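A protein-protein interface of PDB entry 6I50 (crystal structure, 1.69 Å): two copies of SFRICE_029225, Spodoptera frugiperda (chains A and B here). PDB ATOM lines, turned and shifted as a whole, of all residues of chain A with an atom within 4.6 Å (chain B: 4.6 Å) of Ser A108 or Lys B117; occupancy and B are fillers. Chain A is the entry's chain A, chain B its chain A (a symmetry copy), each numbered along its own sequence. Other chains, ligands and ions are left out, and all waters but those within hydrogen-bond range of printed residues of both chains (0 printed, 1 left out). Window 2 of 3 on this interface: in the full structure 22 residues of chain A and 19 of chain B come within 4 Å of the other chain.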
ATOM      1  N   ASP A  83     -13.838 -13.182 -11.786  1.00  0.00           N
ATOM      2  CA  ASP A  83     -14.252 -13.405 -13.167  1.00  0.00           C
ATOM      3  C   ASP A  83     -15.364 -14.439 -13.258  1.00  0.00           C
ATOM      4  O   ASP A  83     -16.239 -14.324 -14.124  1.00  0.00           O
ATOM      5  CB  ASP A  83     -13.062 -13.848 -14.017  1.00  0.00           C
ATOM      6  CG  ASP A  83     -12.147 -12.695 -14.393  1.00  0.00           C
ATOM      7  OD1 ASP A  83     -12.549 -11.525 -14.219  1.00  0.00           O
ATOM      8  OD2 ASP A  83     -11.022 -12.963 -14.866  1.00  0.00           O
ATOM      9  N   THR A  84     -15.352 -15.444 -12.383  1.00  0.00           N
ATOM     10  CA  THR A  84     -16.334 -16.519 -12.404  1.00  0.00           C
ATOM     11  C   THR A  84     -17.059 -16.587 -11.071  1.00  0.00           C
ATOM     12  O   THR A  84     -16.424 -16.569 -10.009  1.00  0.00           O
ATOM     13  CB  THR A  84     -15.670 -17.865 -12.697  1.00  0.00           C
ATOM     14  OG1 THR A  84     -15.021 -17.812 -13.976  1.00  0.00           O
ATOM     15  CG2 THR A  84     -16.695 -18.984 -12.690  1.00  0.00           C
ATOM     16  N   ALA A 106     -23.543 -21.076 -13.365  1.00  0.00           N
ATOM     17  CA  ALA A 106     -22.252 -20.410 -13.496  1.00  0.00           C
ATOM     18  C   ALA A 106     -22.380 -19.201 -14.409  1.00  0.00           C
ATOM     19  O   ALA A 106     -23.156 -19.204 -15.366  1.00  0.00           O
ATOM     20  CB  ALA A 106     -21.174 -21.365 -14.029  1.00  0.00           C
ATOM     21  N   GLN A 107     -21.617 -18.160 -14.094  1.00  0.00           N
ATOM     22  CA  GLN A 107     -21.488 -16.991 -14.952  1.00  0.00           C
ATOM     23  C   GLN A 107     -20.035 -16.552 -14.931  1.00  0.00           C
ATOM     24  O   GLN A 107     -19.389 -16.595 -13.882  1.00  0.00           O
ATOM     25  CB  GLN A 107     -22.401 -15.849 -14.487  1.00  0.00           C
ATOM     26  CG  GLN A 107     -22.751 -14.810 -15.551  1.00  0.00           C
ATOM     27  CD  GLN A 107     -21.664 -13.767 -15.756  1.00  0.00           C
ATOM     28  OE1 GLN A 107     -21.619 -13.096 -16.792  1.00  0.00           O
ATOM     29  NE2 GLN A 107     -20.790 -13.616 -14.765  1.00  0.00           N
ATOM     30  N   SER A 108     -19.515 -16.123 -16.082  1.00  0.00           N
ATOM     31  CA  SER A 108     -18.091 -15.835 -16.173  1.00  0.00           C
ATOM     32  C   SER A 108     -17.815 -14.816 -17.266  1.00  0.00           C
ATOM     33  O   SER A 108     -18.402 -14.872 -18.350  1.00  0.00           O
ATOM     34  CB  SER A 108     -17.281 -17.111 -16.444  1.00  0.00           C
ATOM     35  OG  SER A 108     -15.879 -16.868 -16.340  1.00  0.00           O
ATOM     36  N   SER A 109     -16.917 -13.885 -16.965  1.00  0.00           N
ATOM     37  CA  SER A 109     -16.406 -12.960 -17.962  1.00  0.00           C
ATOM     38  C   SER A 109     -15.030 -12.507 -17.506  1.00  0.00           C
ATOM     39  O   SER A 109     -14.749 -12.461 -16.306  1.00  0.00           O
ATOM     40  CB  SER A 109     -17.333 -11.757 -18.157  1.00  0.00           C
ATOM     41  OG  SER A 109     -17.346 -10.949 -16.994  1.00  0.00           O
ATOM     42  N   TYR B  78     -22.339 -23.907 -20.909  1.00  0.00           N
ATOM     43  CA  TYR B  78     -21.245 -23.760 -21.859  1.00  0.00           C
ATOM     44  C   TYR B  78     -19.908 -23.657 -21.142  1.00  0.00           C
ATOM     45  O   TYR B  78     -19.802 -23.056 -20.069  1.00  0.00           O
ATOM     46  CB  TYR B  78     -21.447 -22.520 -22.734  1.00  0.00           C
ATOM     47  CG  TYR B  78     -22.665 -22.597 -23.625  1.00  0.00           C
ATOM     48  CD1 TYR B  78     -22.600 -23.180 -24.885  1.00  0.00           C
ATOM     49  CD2 TYR B  78     -23.885 -22.087 -23.203  1.00  0.00           C
ATOM     50  CE1 TYR B  78     -23.724 -23.248 -25.699  1.00  0.00           C
ATOM     51  CE2 TYR B  78     -25.003 -22.144 -24.004  1.00  0.00           C
ATOM     52  CZ  TYR B  78     -24.922 -22.726 -25.247  1.00  0.00           C
ATOM     53  OH  TYR B  78     -26.053 -22.774 -26.033  1.00  0.00           O
ATOM     54  N   LEU B  79     -18.886 -24.249 -21.749  1.00  0.00           N
ATOM     55  CA  LEU B  79     -17.495 -24.075 -21.336  1.00  0.00           C
ATOM     56  C   LEU B  79     -16.792 -23.794 -22.657  1.00  0.00           C
ATOM     57  O   LEU B  79     -16.359 -24.713 -23.355  1.00  0.00           O
ATOM     58  CB  LEU B  79     -16.940 -25.303 -20.610  1.00  0.00           C
ATOM     59  CG  LEU B  79     -15.527 -25.133 -20.044  1.00  0.00           C
ATOM     60  CD1 LEU B  79     -15.437 -23.842 -19.247  1.00  0.00           C
ATOM     61  CD2 LEU B  79     -15.136 -26.319 -19.181  1.00  0.00           C
ATOM     62  N   ASP B  80     -16.725 -22.515 -23.017  1.00  0.00           N
ATOM     63  CA  ASP B  80     -16.451 -22.144 -24.393  1.00  0.00           C
ATOM     64  C   ASP B  80     -15.707 -20.820 -24.401  1.00  0.00           C
ATOM     65  O   ASP B  80     -15.799 -20.030 -23.456  1.00  0.00           O
ATOM     66  CB  ASP B  80     -17.755 -22.051 -25.197  1.00  0.00           C
ATOM     67  CG  ASP B  80     -17.523 -22.060 -26.693  1.00  0.00           C
ATOM     68  OD1 ASP B  80     -17.505 -23.154 -27.293  1.00  0.00           O
ATOM     69  OD2 ASP B  80     -17.366 -20.963 -27.268  1.00  0.00           O
ATOM     70  N   HIS B  82     -15.959 -18.561 -27.078  1.00  0.00           N
ATOM     71  CA  HIS B  82     -16.612 -17.542 -27.893  1.00  0.00           C
ATOM     72  C   HIS B  82     -17.210 -16.440 -27.021  1.00  0.00           C
ATOM     73  O   HIS B  82     -17.586 -16.663 -25.866  1.00  0.00           O
ATOM     74  CB  HIS B  82     -17.703 -18.167 -28.762  1.00  0.00           C
ATOM     75  CG  HIS B  82     -17.168 -18.958 -29.912  1.00  0.00           C
ATOM     76  ND1 HIS B  82     -16.908 -20.308 -29.830  1.00  0.00           N
ATOM     77  CD2 HIS B  82     -16.813 -18.582 -31.165  1.00  0.00           C
ATOM     78  CE1 HIS B  82     -16.430 -20.733 -30.985  1.00  0.00           C
ATOM     79  NE2 HIS B  82     -16.357 -19.704 -31.812  1.00  0.00           N
ATOM     80  N   GLN B 107     -26.027 -15.333 -23.802  1.00  0.00           N
ATOM     81  CA  GLN B 107     -25.085 -14.696 -22.892  1.00  0.00           C
ATOM     82  C   GLN B 107     -23.893 -14.225 -23.705  1.00  0.00           C
ATOM     83  O   GLN B 107     -23.456 -14.920 -24.625  1.00  0.00           O
ATOM     84  CB  GLN B 107     -24.633 -15.659 -21.787  1.00  0.00           C
ATOM     85  CG  GLN B 107     -24.092 -15.000 -20.520  1.00  0.00           C
ATOM     86  CD  GLN B 107     -22.640 -14.564 -20.638  1.00  0.00           C
ATOM     87  OE1 GLN B 107     -22.170 -13.716 -19.874  1.00  0.00           O
ATOM     88  NE2 GLN B 107     -21.920 -15.149 -21.592  1.00  0.00           N
ATOM     89  N   SER B 109     -20.134 -11.610 -23.640  1.00  0.00           N
ATOM     90  CA  SER B 109     -19.186 -10.659 -23.086  1.00  0.00           C
ATOM     91  C   SER B 109     -17.985 -10.615 -24.013  1.00  0.00           C
ATOM     92  O   SER B 109     -17.669 -11.602 -24.681  1.00  0.00           O
ATOM     93  CB  SER B 109     -18.757 -11.038 -21.665  1.00  0.00           C
ATOM     94  OG  SER B 109     -17.993 -12.232 -21.681  1.00  0.00           O
ATOM     95  N   ILE B 115     -10.578 -17.175 -24.336  1.00  0.00           N
ATOM     96  CA  ILE B 115     -10.430 -17.796 -23.022  1.00  0.00           C
ATOM     97  C   ILE B 115     -11.671 -18.633 -22.746  1.00  0.00           C
ATOM     98  O   ILE B 115     -12.796 -18.124 -22.817  1.00  0.00           O
ATOM     99  CB  ILE B 115     -10.230 -16.735 -21.930  1.00  0.00           C
ATOM    100  CG1 ILE B 115      -9.112 -15.767 -22.326  1.00  0.00           C
ATOM    101  CG2 ILE B 115      -9.943 -17.395 -20.589  1.00  0.00           C
ATOM    102  CD1 ILE B 115      -7.779 -16.440 -22.579  1.00  0.00           C
ATOM    103  N   ASP B 116     -11.477 -19.917 -22.440  1.00  0.00           N
ATOM    104  CA  ASP B 116     -12.600 -20.773 -22.079  1.00  0.00           C
ATOM    105  C   ASP B 116     -13.184 -20.308 -20.755  1.00  0.00           C
ATOM    106  O   ASP B 116     -12.444 -20.036 -19.804  1.00  0.00           O
ATOM    107  CB  ASP B 116     -12.157 -22.234 -21.968  1.00  0.00           C
ATOM    108  CG  ASP B 116     -11.927 -22.885 -23.318  1.00  0.00           C
ATOM    109  OD1 ASP B 116     -12.552 -22.455 -24.308  1.00  0.00           O
ATOM    110  OD2 ASP B 116     -11.121 -23.838 -23.385  1.00  0.00           O
ATOM    111  N   LYS B 117     -14.510 -20.212 -20.682  1.00  0.00           N
ATOM    112  CA  LYS B 117     -15.118 -19.814 -19.424  1.00  0.00           C
ATOM    113  C   LYS B 117     -16.494 -20.432 -19.296  1.00  0.00           C
ATOM    114  O   LYS B 117     -17.167 -20.677 -20.307  1.00  0.00           O
ATOM    115  CB  LYS B 117     -15.211 -18.289 -19.287  1.00  0.00           C
ATOM    116  CG  LYS B 117     -15.955 -17.600 -20.389  1.00  0.00           C
ATOM    117  CD  LYS B 117     -15.395 -16.204 -20.549  1.00  0.00           C
ATOM    118  CE  LYS B 117     -15.374 -15.795 -22.003  1.00  0.00           C
ATOM    119  NZ  LYS B 117     -16.752 -15.716 -22.562  1.00  0.00           N
ATOM    120  N   PRO B 118     -16.944 -20.699 -18.067  1.00  0.00           N
ATOM    121  CA  PRO B 118     -18.230 -21.367 -17.862  1.00  0.00           C
ATOM    122  C   PRO B 118     -19.390 -20.388 -17.792  1.00  0.00           C
ATOM    123  O   PRO B 118     -19.296 -19.369 -17.101  1.00  0.00           O
ATOM    124  CB  PRO B 118     -18.030 -22.082 -16.521  1.00  0.00           C
ATOM    125  CG  PRO B 118     -17.084 -21.193 -15.783  1.00  0.00           C
ATOM    126  CD  PRO B 118     -16.184 -20.556 -16.813  1.00  0.00           C
ATOM    127  N   ASN B 119     -20.482 -20.694 -18.491  1.00  0.00           N
ATOM    128  CA  ASN B 119     -21.698 -19.885 -18.448  1.00  0.00           C
ATOM    129  C   ASN B 119     -22.886 -20.807 -18.664  1.00  0.00           C
ATOM    130  O   ASN B 119     -22.977 -21.449 -19.712  1.00  0.00           O
ATOM    131  CB  ASN B 119     -21.687 -18.797 -19.527  1.00  0.00           C
ATOM    132  CG  ASN B 119     -20.905 -17.578 -19.119  1.00  0.00           C
ATOM    133  OD1 ASN B 119     -21.333 -16.814 -18.253  1.00  0.00           O
ATOM    134  ND2 ASN B 119     -19.755 -17.374 -19.750  1.00  0.00           N
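Gln A107 touches its own counterpart, Gln B107. Ser A109 touches its own counterpart, Ser B109. Positions printed for both chains: 107 and 109. Of the 9 pairs that touch across the chains among the printed residues, 2 have their exchanged pair printed and touching as well.
O of Asp A83 sits close to OG of Ser A108 (3.4 Å). O of Asp A83 lies within hydrogen-bond range of N of Ser A109, 3.0 Å away. OG1 of Thr A84 lies within hydrogen-bond range of OG of Ser A108. O of Asn B119 lies within hydrogen-bond range of N of Tyr B78. N of Lys B117 is in hydrogen-bond range of O of Asp B80 (3.1 Å).
Thr A84 touches Pro B118. Ala A106 touches Asn B119. Gln A107 touches Pro B118 (C to O, 3.6 Å). Gln A107 touches Asn B119. CB of Lys B117 touches OG of Ser A108, at 3.3 Å. Ser A109 touches Ser B109 (CB to OG, 3.6 Å).
Of chain B, only Lys B117 (3.3 Å), Pro B118 (3.1 Å) and Asn B119 (2.9 Å) come within 4 Å of Ser A108. Printed residues of chain A within 4 Å of Lys B117: Ser A108 (3.3 Å). Printed residues of chain B within 4 Å of Thr A84: Pro B118 (3.8 Å). Of the printed residues of chain A, Gln B107 touches Gln A107.
OE1 of Gln B107 lies close to OE1 of Gln A107 (3.2 Å). The backbone NH of Ser A108 sits close to the backbone carbonyl oxygen of Pro B118, at 3.4 Å. The backbone NH of Ser A108 sits at hydrogen-bond distance from the side-chain amide oxygen of Asn B119 (2.9 Å).
Of the 11 printed residues of chain B, 5 touch a printed residue of chain A. Among the printed residues, 9 pairs touch across the chains.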
